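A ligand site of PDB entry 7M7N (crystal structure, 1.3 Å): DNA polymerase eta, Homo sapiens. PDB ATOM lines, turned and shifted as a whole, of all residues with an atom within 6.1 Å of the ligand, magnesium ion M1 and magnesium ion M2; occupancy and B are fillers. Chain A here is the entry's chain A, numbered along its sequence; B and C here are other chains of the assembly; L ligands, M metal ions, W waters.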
ATOM      1  N   ASP A  16      -2.661   3.712   6.868  1.00  0.00           N
ATOM      2  CA  ASP A  16      -1.568   4.653   7.102  1.00  0.00           C
ATOM      3  C   ASP A  16      -2.099   6.075   7.078  1.00  0.00           C
ATOM      4  O   ASP A  16      -2.744   6.499   6.106  1.00  0.00           O
ATOM      5  CB  ASP A  16      -0.468   4.512   6.049  1.00  0.00           C
ATOM      6  CG  ASP A  16       0.715   5.372   6.346  1.00  0.00           C
ATOM      7  OD1 ASP A  16       0.601   6.592   6.119  1.00  0.00           O
ATOM      8  OD2 ASP A  16       1.733   4.833   6.812  1.00  0.00           O
ATOM      9  N   MET A  17      -1.829   6.810   8.158  1.00  0.00           N
ATOM     10  CA  MET A  17      -2.378   8.156   8.279  1.00  0.00           C
ATOM     11  C   MET A  17      -1.776   9.102   7.257  1.00  0.00           C
ATOM     12  O   MET A  17      -0.595   9.015   6.895  1.00  0.00           O
ATOM     13  CB  MET A  17      -2.110   8.697   9.694  1.00  0.00           C
ATOM     14  CG  MET A  17      -2.607   7.788  10.823  1.00  0.00           C
ATOM     15  SD  MET A  17      -4.347   7.337  10.708  1.00  0.00           S
ATOM     16  CE  MET A  17      -5.090   8.929  10.871  1.00  0.00           C
ATOM     17  N   ASP A  18      -2.601  10.015   6.743  1.00  0.00           N
ATOM     18  CA  ASP A  18      -2.107  11.001   5.792  1.00  0.00           C
ATOM     19  C   ASP A  18      -1.357  12.105   6.529  1.00  0.00           C
ATOM     20  O   ASP A  18      -1.842  12.601   7.569  1.00  0.00           O
ATOM     21  CB  ASP A  18      -3.245  11.594   4.981  1.00  0.00           C
ATOM     22  CG  ASP A  18      -3.969  10.563   4.127  1.00  0.00           C
ATOM     23  OD1 ASP A  18      -3.365   9.553   3.719  1.00  0.00           O
ATOM     24  OD2 ASP A  18      -5.165  10.777   3.856  1.00  0.00           O
ATOM     25  N   CYS A  19      -0.177  12.464   6.026  1.00  0.00           N
ATOM     26  CA  CYS A  19       0.693  13.496   6.618  1.00  0.00           C
ATOM     27  C   CYS A  19       0.494  13.628   8.125  1.00  0.00           C
ATOM     28  O   CYS A  19       0.103  14.691   8.625  1.00  0.00           O
ATOM     29  CB  CYS A  19       0.570  14.834   5.874  1.00  0.00           C
ATOM     30  SG  CYS A  19      -1.097  15.531   5.716  1.00  0.00           S
ATOM     31  N   PHE A  20       0.777  12.554   8.857  1.00  0.00           N
ATOM     32  CA  PHE A  20       0.205  12.362  10.187  1.00  0.00           C
ATOM     33  C   PHE A  20       0.510  13.514  11.141  1.00  0.00           C
ATOM     34  O   PHE A  20      -0.420  14.091  11.738  1.00  0.00           O
ATOM     35  CB  PHE A  20       0.640  11.026  10.769  1.00  0.00           C
ATOM     36  CG  PHE A  20       0.042  10.726  12.111  1.00  0.00           C
ATOM     37  CD1 PHE A  20      -1.312  10.886  12.322  1.00  0.00           C
ATOM     38  CD2 PHE A  20       0.844  10.265  13.139  1.00  0.00           C
ATOM     39  CE1 PHE A  20      -1.874  10.605  13.559  1.00  0.00           C
ATOM     40  CE2 PHE A  20       0.302   9.975  14.377  1.00  0.00           C
ATOM     41  CZ  PHE A  20      -1.065  10.138  14.585  1.00  0.00           C
ATOM     42  N   PHE A  21       1.795  13.852  11.359  1.00  0.00           N
ATOM     43  CA  PHE A  21       2.057  14.872  12.379  1.00  0.00           C
ATOM     44  C   PHE A  21       1.450  16.209  11.985  1.00  0.00           C
ATOM     45  O   PHE A  21       1.020  16.993  12.860  1.00  0.00           O
ATOM     46  CB  PHE A  21       3.555  15.073  12.634  1.00  0.00           C
ATOM     47  CG  PHE A  21       4.266  13.916  13.312  1.00  0.00           C
ATOM     48  CD1 PHE A  21       3.682  12.672  13.489  1.00  0.00           C
ATOM     49  CD2 PHE A  21       5.570  14.098  13.745  1.00  0.00           C
ATOM     50  CE1 PHE A  21       4.394  11.617  14.102  1.00  0.00           C
ATOM     51  CE2 PHE A  21       6.278  13.078  14.370  1.00  0.00           C
ATOM     52  CZ  PHE A  21       5.700  11.835  14.523  1.00  0.00           C
ATOM     53  N   VAL A  22       1.382  16.498  10.682  1.00  0.00           N
ATOM     54  CA  VAL A  22       0.714  17.719  10.228  1.00  0.00           C
ATOM     55  C   VAL A  22      -0.750  17.713  10.639  1.00  0.00           C
ATOM     56  O   VAL A  22      -1.277  18.707  11.141  1.00  0.00           O
ATOM     57  CB  VAL A  22       0.897  17.904   8.712  1.00  0.00           C
ATOM     58  CG1 VAL A  22      -0.045  18.978   8.202  1.00  0.00           C
ATOM     59  CG2 VAL A  22       2.348  18.232   8.402  1.00  0.00           C
ATOM     60  N   GLN A  41      11.469  20.189  13.516  1.00  0.00           N
ATOM     61  CA  GLN A  41      12.173  19.985  14.774  1.00  0.00           C
ATOM     62  C   GLN A  41      13.307  20.988  14.847  1.00  0.00           C
ATOM     63  O   GLN A  41      14.117  21.078  13.920  1.00  0.00           O
ATOM     64  CB  GLN A  41      12.736  18.566  14.877  1.00  0.00           C
ATOM     65  CG  GLN A  41      11.692  17.549  15.235  1.00  0.00           C
ATOM     66  CD  GLN A  41      12.228  16.138  15.361  1.00  0.00           C
ATOM     67  OE1 GLN A  41      11.817  15.402  16.247  1.00  0.00           O
ATOM     68  NE2 GLN A  41      13.135  15.746  14.464  1.00  0.00           N
ATOM     69  N   ILE A  51       9.902  17.126   9.242  1.00  0.00           N
ATOM     70  CA  ILE A  51       9.602  15.700   9.381  1.00  0.00           C
ATOM     71  C   ILE A  51       8.231  15.304   8.850  1.00  0.00           C
ATOM     72  O   ILE A  51       7.955  14.091   8.782  1.00  0.00           O
ATOM     73  CB  ILE A  51       9.821  15.183  10.826  1.00  0.00           C
ATOM     74  CG1 ILE A  51       8.937  15.916  11.838  1.00  0.00           C
ATOM     75  CG2 ILE A  51      11.312  15.227  11.194  1.00  0.00           C
ATOM     76  CD1 ILE A  51       9.023  15.332  13.248  1.00  0.00           C
ATOM     77  N   ALA A  52       7.371  16.249   8.468  1.00  0.00           N
ATOM     78  CA  ALA A  52       6.075  15.911   7.877  1.00  0.00           C
ATOM     79  C   ALA A  52       5.582  17.115   7.091  1.00  0.00           C
ATOM     80  O   ALA A  52       5.847  18.260   7.459  1.00  0.00           O
ATOM     81  CB  ALA A  52       5.050  15.533   8.962  1.00  0.00           C
ATOM     82  N   VAL A  53       4.848  16.847   5.995  1.00  0.00           N
ATOM     83  CA  VAL A  53       4.511  17.861   5.000  1.00  0.00           C
ATOM     84  C   VAL A  53       3.078  17.635   4.525  1.00  0.00           C
ATOM     85  O   VAL A  53       2.732  16.534   4.096  1.00  0.00           O
ATOM     86  CB  VAL A  53       5.462  17.809   3.777  1.00  0.00           C
ATOM     87  CG1 VAL A  53       5.162  18.938   2.819  1.00  0.00           C
ATOM     88  CG2 VAL A  53       6.930  17.817   4.213  1.00  0.00           C
ATOM     89  N   TYR A  55      -0.170  17.855   2.022  1.00  0.00           N
ATOM     90  CA  TYR A  55      -0.235  17.633   0.573  1.00  0.00           C
ATOM     91  C   TYR A  55      -0.213  18.941  -0.207  1.00  0.00           C
ATOM     92  O   TYR A  55       0.413  19.018  -1.290  1.00  0.00           O
ATOM     93  CB  TYR A  55      -1.411  16.703   0.238  1.00  0.00           C
ATOM     94  CG  TYR A  55      -1.069  15.273   0.543  1.00  0.00           C
ATOM     95  CD1 TYR A  55      -1.135  14.769   1.840  1.00  0.00           C
ATOM     96  CD2 TYR A  55      -0.595  14.432  -0.453  1.00  0.00           C
ATOM     97  CE1 TYR A  55      -0.774  13.472   2.123  1.00  0.00           C
ATOM     98  CE2 TYR A  55      -0.245  13.132  -0.190  1.00  0.00           C
ATOM     99  CZ  TYR A  55      -0.323  12.647   1.105  1.00  0.00           C
ATOM    100  OH  TYR A  55       0.044  11.350   1.364  1.00  0.00           O
ATOM    101  N   ARG A  58       3.368  19.722  -0.430  1.00  0.00           N
ATOM    102  CA  ARG A  58       4.058  18.823  -1.352  1.00  0.00           C
ATOM    103  C   ARG A  58       3.902  19.284  -2.791  1.00  0.00           C
ATOM    104  O   ARG A  58       4.800  19.063  -3.610  1.00  0.00           O
ATOM    105  CB  ARG A  58       3.564  17.388  -1.211  1.00  0.00           C
ATOM    106  CG  ARG A  58       3.743  16.793   0.171  1.00  0.00           C
ATOM    107  CD  ARG A  58       3.292  15.339   0.246  1.00  0.00           C
ATOM    108  NE  ARG A  58       3.142  14.945   1.652  1.00  0.00           N
ATOM    109  CZ  ARG A  58       2.979  13.698   2.086  1.00  0.00           C
ATOM    110  NH1 ARG A  58       2.954  12.677   1.243  1.00  0.00           N
ATOM    111  NH2 ARG A  58       2.843  13.478   3.394  1.00  0.00           N
ATOM    112  N   ARG A  64      10.098  15.987   3.273  1.00  0.00           N
ATOM    113  CA  ARG A  64      10.764  15.603   4.509  1.00  0.00           C
ATOM    114  C   ARG A  64      12.274  15.735   4.319  1.00  0.00           C
ATOM    115  O   ARG A  64      12.799  15.593   3.214  1.00  0.00           O
ATOM    116  CB  ARG A  64      10.417  14.149   4.821  1.00  0.00           C
ATOM    117  CG  ARG A  64      10.993  13.565   6.093  1.00  0.00           C
ATOM    118  CD  ARG A  64      10.446  12.162   6.317  1.00  0.00           C
ATOM    119  NE  ARG A  64      11.192  11.139   5.596  1.00  0.00           N
ATOM    120  CZ  ARG A  64      10.713   9.931   5.312  1.00  0.00           C
ATOM    121  NH1 ARG A  64       9.477   9.600   5.672  1.00  0.00           N
ATOM    122  NH2 ARG A  64      11.465   9.055   4.655  1.00  0.00           N
ATOM    123  N   SER A 116       4.031   1.288  12.618  1.00  0.00           N
ATOM    124  CA  SER A 116       4.763   2.516  12.878  1.00  0.00           C
ATOM    125  C   SER A 116       3.857   3.409  13.690  1.00  0.00           C
ATOM    126  O   SER A 116       2.698   3.079  13.947  1.00  0.00           O
ATOM    127  CB  SER A 116       5.197   3.226  11.585  1.00  0.00           C
ATOM    128  OG  SER A 116       4.179   4.083  11.076  1.00  0.00           O
ATOM    129  N   ILE A 117       4.380   4.589  14.048  1.00  0.00           N
ATOM    130  CA  ILE A 117       3.571   5.555  14.781  1.00  0.00           C
ATOM    131  C   ILE A 117       2.265   5.874  14.065  1.00  0.00           C
ATOM    132  O   ILE A 117       1.284   6.274  14.704  1.00  0.00           O
ATOM    133  CB  ILE A 117       4.389   6.820  15.101  1.00  0.00           C
ATOM    134  CG1 ILE A 117       3.708   7.618  16.225  1.00  0.00           C
ATOM    135  CG2 ILE A 117       4.586   7.650  13.828  1.00  0.00           C
ATOM    136  CD1 ILE A 117       4.588   8.707  16.813  1.00  0.00           C
ATOM    137  N   ASP A 118       2.203   5.715  12.732  1.00  0.00           N
ATOM    138  CA  ASP A 118       0.992   6.120  12.012  1.00  0.00           C
ATOM    139  C   ASP A 118       0.398   5.006  11.179  1.00  0.00           C
ATOM    140  O   ASP A 118      -0.404   5.296  10.282  1.00  0.00           O
ATOM    141  CB  ASP A 118       1.219   7.381  11.177  1.00  0.00           C
ATOM    142  CG  ASP A 118       1.634   7.087   9.742  1.00  0.00           C
ATOM    143  OD1 ASP A 118       2.446   6.149   9.519  1.00  0.00           O
ATOM    144  OD2 ASP A 118       1.131   7.808   8.854  1.00  0.00           O
ATOM    145  N   GLU A 119       0.765   3.745  11.427  1.00  0.00           N
ATOM    146  CA  GLU A 119       0.166   2.734  10.553  1.00  0.00           C
ATOM    147  C   GLU A 119       0.087   1.397  11.251  1.00  0.00           C
ATOM    148  O   GLU A 119       0.930   1.063  12.103  1.00  0.00           O
ATOM    149  CB  GLU A 119       0.906   2.576   9.224  1.00  0.00           C
ATOM    150  CG  GLU A 119       2.231   1.866   9.300  1.00  0.00           C
ATOM    151  CD  GLU A 119       3.174   2.399   8.253  1.00  0.00           C
ATOM    152  OE1 GLU A 119       3.435   1.699   7.249  1.00  0.00           O
ATOM    153  OE2 GLU A 119       3.637   3.547   8.417  1.00  0.00           O
ATOM    154  N   LYS A 227       0.525  -2.812   1.900  1.00  0.00           N
ATOM    155  CA  LYS A 227       1.332  -1.612   2.048  1.00  0.00           C
ATOM    156  C   LYS A 227       1.535  -0.913   0.701  1.00  0.00           C
ATOM    157  O   LYS A 227       1.371   0.312   0.592  1.00  0.00           O
ATOM    158  CB  LYS A 227       2.681  -1.961   2.690  1.00  0.00           C
ATOM    159  CG  LYS A 227       3.678  -0.788   2.766  1.00  0.00           C
ATOM    160  CD  LYS A 227       3.193   0.364   3.670  1.00  0.00           C
ATOM    161  CE  LYS A 227       4.321   1.361   3.855  1.00  0.00           C
ATOM    162  NZ  LYS A 227       3.941   2.556   4.659  1.00  0.00           N
ATOM    163  N   LYS A 234      -3.011   7.557  -2.134  1.00  0.00           N
ATOM    164  CA  LYS A 234      -2.950   8.586  -1.100  1.00  0.00           C
ATOM    165  C   LYS A 234      -3.092   9.967  -1.739  1.00  0.00           C
ATOM    166  O   LYS A 234      -2.559  10.203  -2.825  1.00  0.00           O
ATOM    167  CB  LYS A 234      -1.590   8.530  -0.411  1.00  0.00           C
ATOM    168  CG  LYS A 234      -1.638   7.853   0.917  1.00  0.00           C
ATOM    169  CD  LYS A 234      -0.294   7.828   1.599  1.00  0.00           C
ATOM    170  CE  LYS A 234      -0.423   7.109   2.931  1.00  0.00           C
ATOM    171  NZ  LYS A 234      -0.977   7.986   4.004  1.00  0.00           N
ATOM    172  N   PRO A 235      -3.741  10.927  -1.058  1.00  0.00           N
ATOM    173  CA  PRO A 235      -4.316  10.798   0.293  1.00  0.00           C
ATOM    174  C   PRO A 235      -5.820  10.525   0.284  1.00  0.00           C
ATOM    175  O   PRO A 235      -6.486  10.664  -0.748  1.00  0.00           O
ATOM    176  CB  PRO A 235      -4.069  12.184   0.881  1.00  0.00           C
ATOM    177  CG  PRO A 235      -4.229  13.097  -0.299  1.00  0.00           C
ATOM    178  CD  PRO A 235      -3.742  12.325  -1.513  1.00  0.00           C
ATOM    179  P    DA B   7      13.079  -0.183   2.869  1.00  0.00           P
ATOM    180  OP1  DA B   7      12.217  -0.958   1.952  1.00  0.00           O
ATOM    181  OP2  DA B   7      14.048   0.767   2.327  1.00  0.00           O
ATOM    182  O5'  DA B   7      12.201   0.670   3.899  1.00  0.00           O
ATOM    183  C5'  DA B   7      11.273   0.049   4.712  1.00  0.00           C
ATOM    184  C4'  DA B   7      10.805   1.002   5.783  1.00  0.00           C
ATOM    185  O4'  DA B   7      11.884   1.280   6.709  1.00  0.00           O
ATOM    186  C3'  DA B   7      10.336   2.379   5.273  1.00  0.00           C
ATOM    187  O3'  DA B   7       8.965   2.491   5.558  1.00  0.00           O
ATOM    188  C2'  DA B   7      11.164   3.376   6.073  1.00  0.00           C
ATOM    189  C1'  DA B   7      11.650   2.523   7.249  1.00  0.00           C
ATOM    190  N9   DA B   7      12.880   3.016   7.843  1.00  0.00           N
ATOM    191  C8   DA B   7      14.082   3.186   7.227  1.00  0.00           C
ATOM    192  N7   DA B   7      15.003   3.686   8.005  1.00  0.00           N
ATOM    193  C5   DA B   7      14.348   3.874   9.218  1.00  0.00           C
ATOM    194  C6   DA B   7      14.773   4.381  10.452  1.00  0.00           C
ATOM    195  N6   DA B   7      16.019   4.822  10.684  1.00  0.00           N
ATOM    196  N1   DA B   7      13.866   4.446  11.451  1.00  0.00           N
ATOM    197  C2   DA B   7      12.613   4.012  11.223  1.00  0.00           C
ATOM    198  N3   DA B   7      12.100   3.505  10.101  1.00  0.00           N
ATOM    199  C4   DA B   7      13.036   3.475   9.127  1.00  0.00           C
ATOM    200  F   AF2 B   8       6.632   6.183  10.980  1.00  0.00           F
ATOM    201  P   AF2 B   8       8.065   3.700   5.050  1.00  0.00           P
ATOM    202  N1  AF2 B   8      12.671   8.218  11.523  1.00  0.00           N
ATOM    203  C2  AF2 B   8      11.503   7.917  12.103  1.00  0.00           C
ATOM    204  N3  AF2 B   8      10.471   7.246  11.612  1.00  0.00           N
ATOM    205  C4  AF2 B   8      10.723   6.847  10.353  1.00  0.00           C
ATOM    206  C5  AF2 B   8      11.863   7.090   9.613  1.00  0.00           C
ATOM    207  C6  AF2 B   8      12.894   7.806  10.256  1.00  0.00           C
ATOM    208  N6  AF2 B   8      14.054   8.113   9.679  1.00  0.00           N
ATOM    209  N7  AF2 B   8      11.763   6.536   8.341  1.00  0.00           N
ATOM    210  C8  AF2 B   8      10.577   5.991   8.342  1.00  0.00           C
ATOM    211  N9  AF2 B   8       9.867   6.172   9.502  1.00  0.00           N
ATOM    212  C1' AF2 B   8       8.598   5.570   9.889  1.00  0.00           C
ATOM    213  OP2 AF2 B   8       8.855   4.726   4.329  1.00  0.00           O
ATOM    214  C2' AF2 B   8       7.323   6.407   9.812  1.00  0.00           C
ATOM    215  OP1 AF2 B   8       6.887   3.105   4.394  1.00  0.00           O
ATOM    216  C3' AF2 B   8       6.550   5.732   8.688  1.00  0.00           C
ATOM    217  O3' AF2 B   8       5.157   5.790   8.937  1.00  0.00           O
ATOM    218  C4' AF2 B   8       7.026   4.286   8.739  1.00  0.00           C
ATOM    219  O4' AF2 B   8       8.419   4.408   9.105  1.00  0.00           O
ATOM    220  C5' AF2 B   8       6.933   3.558   7.427  1.00  0.00           C
ATOM    221  O5' AF2 B   8       7.583   4.357   6.414  1.00  0.00           O
ATOM    222  P    DT C   4      20.801  15.469  11.613  1.00  0.00           P
ATOM    223  OP1  DT C   4      21.813  16.146  12.456  1.00  0.00           O
ATOM    224  OP2  DT C   4      21.033  14.128  11.050  1.00  0.00           O
ATOM    225  O5'  DT C   4      19.470  15.360  12.493  1.00  0.00           O
ATOM    226  C5'  DT C   4      18.930  16.506  13.109  1.00  0.00           C
ATOM    227  C4'  DT C   4      17.784  16.114  14.020  1.00  0.00           C
ATOM    228  O4'  DT C   4      16.745  15.471  13.247  1.00  0.00           O
ATOM    229  C3'  DT C   4      18.149  15.141  15.137  1.00  0.00           C
ATOM    230  O3'  DT C   4      17.364  15.440  16.256  1.00  0.00           O
ATOM    231  C2'  DT C   4      17.779  13.785  14.527  1.00  0.00           C
ATOM    232  C1'  DT C   4      16.548  14.146  13.713  1.00  0.00           C
ATOM    233  N1   DT C   4      16.276  13.283  12.533  1.00  0.00           N
ATOM    234  C2   DT C   4      14.979  12.864  12.341  1.00  0.00           C
ATOM    235  O2   DT C   4      14.090  13.126  13.117  1.00  0.00           O
ATOM    236  N3   DT C   4      14.779  12.109  11.232  1.00  0.00           N
ATOM    237  C4   DT C   4      15.712  11.751  10.279  1.00  0.00           C
ATOM    238  O4   DT C   4      15.409  11.061   9.302  1.00  0.00           O
ATOM    239  C5   DT C   4      17.057  12.231  10.523  1.00  0.00           C
ATOM    240  C7   DT C   4      18.172  11.901   9.566  1.00  0.00           C
ATOM    241  C6   DT C   4      17.266  12.985  11.621  1.00  0.00           C
ATOM    242  P    DT C   5      17.565  14.643  17.635  1.00  0.00           P
ATOM    243  OP1  DT C   5      17.385  15.645  18.704  1.00  0.00           O
ATOM    244  OP2  DT C   5      18.803  13.823  17.607  1.00  0.00           O
ATOM    245  O5'  DT C   5      16.321  13.628  17.643  1.00  0.00           O
ATOM    246  C5'  DT C   5      14.994  14.118  17.739  1.00  0.00           C
ATOM    247  C4'  DT C   5      14.015  12.972  17.756  1.00  0.00           C
ATOM    248  O4'  DT C   5      14.002  12.344  16.445  1.00  0.00           O
ATOM    249  C3'  DT C   5      14.352  11.842  18.740  1.00  0.00           C
ATOM    250  O3'  DT C   5      13.142  11.360  19.321  1.00  0.00           O
ATOM    251  C2'  DT C   5      15.008  10.795  17.835  1.00  0.00           C
ATOM    252  C1'  DT C   5      14.144  10.955  16.603  1.00  0.00           C
ATOM    253  N1   DT C   5      14.710  10.402  15.351  1.00  0.00           N
ATOM    254  C2   DT C   5      13.843   9.879  14.430  1.00  0.00           C
ATOM    255  O2   DT C   5      12.645   9.840  14.608  1.00  0.00           O
ATOM    256  N3   DT C   5      14.434   9.398  13.296  1.00  0.00           N
ATOM    257  C4   DT C   5      15.778   9.402  12.985  1.00  0.00           C
ATOM    258  O4   DT C   5      16.207   8.944  11.928  1.00  0.00           O
ATOM    259  C5   DT C   5      16.641   9.979  13.986  1.00  0.00           C
ATOM    260  C7   DT C   5      18.124  10.035  13.766  1.00  0.00           C
ATOM    261  C6   DT C   5      16.073  10.458  15.114  1.00  0.00           C
HETATM  262  N1  LIG L   1      12.156  11.311  10.815  1.00  0.00           N
HETATM  263  C1  LIG L   1      11.279  11.584  11.789  1.00  0.00           C
HETATM  264  N2  LIG L   1       9.954  11.414  11.805  1.00  0.00           N
HETATM  265  C2  LIG L   1       9.539  10.872  10.652  1.00  0.00           C
HETATM  266  C3  LIG L   1      10.307  10.527   9.570  1.00  0.00           C
HETATM  267  C4  LIG L   1      11.689  10.770   9.670  1.00  0.00           C
HETATM  268  N3  LIG L   1      12.523  10.475   8.677  1.00  0.00           N
HETATM  269  N4  LIG L   1       9.512   9.993   8.561  1.00  0.00           N
HETATM  270  C5  LIG L   1       8.301  10.031   9.045  1.00  0.00           C
HETATM  271  N5  LIG L   1       8.249  10.548  10.312  1.00  0.00           N
HETATM  272  P1  LIG L   1       4.768   8.461   7.076  1.00  0.00           P
HETATM  273  P2  LIG L   1       3.221  10.911   6.611  1.00  0.00           P
HETATM  274  P3  LIG L   1       1.907  10.125   4.123  1.00  0.00           P
HETATM  275  C6  LIG L   1       7.096  10.754  11.172  1.00  0.00           C
HETATM  276  O1  LIG L   1       3.589   7.618   7.164  1.00  0.00           O
HETATM  277  O2  LIG L   1       2.160  10.320   7.412  1.00  0.00           O
HETATM  278  O3  LIG L   1       1.854   8.818   4.853  1.00  0.00           O
HETATM  279  C7  LIG L   1       6.288  11.984  10.780  1.00  0.00           C
HETATM  280  O4  LIG L   1       5.933   7.675   6.415  1.00  0.00           O
HETATM  281  O5  LIG L   1       3.634  12.298   7.182  1.00  0.00           O
HETATM  282  O6  LIG L   1       0.543  10.704   3.891  1.00  0.00           O
HETATM  283  C8  LIG L   1       5.160  11.410   9.935  1.00  0.00           C
HETATM  284  O7  LIG L   1       3.984  12.209   9.996  1.00  0.00           O
HETATM  285  N6  LIG L   1       4.497   9.910   6.377  1.00  0.00           N
HETATM  286  O8  LIG L   1       2.643  11.140   5.128  1.00  0.00           O
HETATM  287  O9  LIG L   1       2.737  10.061   2.873  1.00  0.00           O
HETATM  288  C9  LIG L   1       4.933  10.055  10.591  1.00  0.00           C
HETATM  289  O10 LIG L   1       6.228   9.630  11.050  1.00  0.00           O
HETATM  290  C10 LIG L   1       4.379   9.005   9.665  1.00  0.00           C
HETATM  291  O11 LIG L   1       5.298   8.798   8.560  1.00  0.00           O
HETATM  292 MG    MG M   1       1.418   8.320   6.904  1.00  0.00          MG
HETATM  293 MG    MG M   2       3.391   5.555   7.780  1.00  0.00          MG
HETATM  294  O   HOH W   1       4.479   5.229   6.012  1.00  0.00           O
HETATM  295  O   HOH W   2       2.990   6.487   4.022  1.00  0.00           O
HETATM  296  O   HOH W   3       5.408  10.396   3.409  1.00  0.00           O
HETATM  297  O   HOH W   4       6.959  12.159   6.692  1.00  0.00           O
HETATM  298  O   HOH W   5       9.219  11.504  14.587  1.00  0.00           O
HETATM  299  O   HOH W   6       7.996   7.919  12.948  1.00  0.00           O
HETATM  300  O   HOH W   7       4.779  14.018   5.536  1.00  0.00           O
HETATM  301  O   HOH W   8       7.574   7.282   4.308  1.00  0.00           O
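Ser 116 touches magnesium ion M2 (OG to MG, 3.7 Å).
The nearest printed residue that does not touch magnesium ion M2 is Lys 227 (4.4 Å).
Magnesium ion M2 is bound by OD2 of Asp 16, at 2.1 Å.
Magnesium ion M2 is bound by OD1 of Asp 118 (2.1 Å).
Magnesium ion M2 is bound by water W1, at 2.1 Å.
OE2 of Glu 119 binds magnesium ion M2 (2.1 Å).
O3' of AF2 8 of chain B is bound to magnesium ion M2, 2.1 Å away.
O1 of the ligand is bound to magnesium ion M2 (2.2 Å).
Water W1 lies within hydrogen-bond range of an oxygen (O4) of the ligand (2.9 Å), the side-chain amino group of Lys 227 (3.0 Å) and O5' of AF2 8 of chain B (3.2 Å).
Water W7 lies within hydrogen-bond range of O5 of the ligand (2.6 Å), N of Val 53 (2.9 Å) and NH2 of Arg 58 (2.9 Å).
Water W8 lies within hydrogen-bond range of O4 of the ligand (2.7 Å), OP2 of AF2 8 of chain B (2.9 Å) and NH1 of Arg 64 (3.3 Å).
Water W6 bridges N3 of AF2 8 of chain B (2.9 Å) and an oxygen (O10) of the ligand (3.1 Å).
Water W4 lies within hydrogen-bond range of O of Ile 51 and N6 of the ligand.
The backbone NH of Asp 118 lies close to the side-chain hydroxyl of Ser 116.
The side-chain amino group of Lys 234 is in hydrogen-bond range of the backbone carbonyl oxygen of Asp 16, at 3.1 Å.
The side-chain hydroxyl (OG) of Ser 116 sits close to the backbone NH (N) of Glu 119 (3.4 Å).
The side-chain amino group of Lys 227 lies within salt-bridge range of the side-chain carboxylate of Glu 119 (2.8 Å).
O3' of AF2 8 of chain B sits close to the side-chain hydroxyl (OG) of Ser 116.
NZ of Lys 234 lies close to O of Met 17.
OH of Tyr 55 sits at hydrogen-bond distance from NH1 of Arg 58.
NE2 of Gln 41 lies within hydrogen-bond range of O2 of DT 4 of chain C (3.1 Å).
Merely in contact with magnesium ion M1: Lys 234 (3.8 Å).
Of the 25 residues printed, 4 come within 4 Å of magnesium ion M1.
Along chain A the residues within 4 Å of magnesium ion M1 span positions 16 to 234.
Magnesium ion M1 is bound by OD2 of Asp 118.
OD1 of Asp 16 binds magnesium ion M1 (2.1 Å).
The backbone carbonyl oxygen (O) of Met 17 is bound to magnesium ion M1, at 2.1 Å.
Magnesium ion M1 is bound by O3 of the ligand, at 2.2 Å.
Magnesium ion M1 is bound by an oxygen (O2) of the ligand, 2.2 Å away.
O1 of the ligand binds magnesium ion M1.
N6 of AF2 8 of chain B is in hydrogen-bond range of a nitrogen (N3) of the ligand (3.0 Å).
The side-chain hydroxyl of Tyr 55 lies within hydrogen-bond range of an oxygen (O6) of the ligand.
N3 of the ligand sits at hydrogen-bond distance from O4 of DT 4 of chain C (3.0 Å).
An oxygen (O6) of the ligand sits at hydrogen-bond distance from the backbone NH (N) of Cys 19, at 2.9 Å.
N4 of the ligand sits at hydrogen-bond distance from NH1 of Arg 64 (2.9 Å).
The guanidinium group of Arg 58 lies within salt-bridge range of an oxygen (O9) of the ligand (3.1 Å).
O5 of the ligand lies within hydrogen-bond range of N of Phe 20.
An oxygen (O7) of the ligand sits at hydrogen-bond distance from the backbone NH (N) of Phe 21 (3.1 Å).
NZ of Lys 234 is in salt-bridge range of O6 of the ligand, 3.1 Å away.
Asp 18 touches the ligand.
Ile 51 touches the ligand (O to C7, 3.3 Å).
Ala 52 touches the ligand.
Ile 117 touches the ligand.
DT 5 of chain C touches the ligand.
Hydrophobic or aromatic side chains within 4 Å of the ligand: Phe 20, Phe 21, Ile 51, Ala 52, Tyr 55 and Ile 117.
17 residues have an atom within 4 Å of the ligand: Asp 16, Met 17, Asp 18, Cys 19, Phe 20, Phe 21, Ile 51, Ala 52, Tyr 55, Arg 58, Arg 64, Ile 117, Asp 118, Lys 234, AF2 8 of chain B, DT 4 of chain C and DT 5 of chain C.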
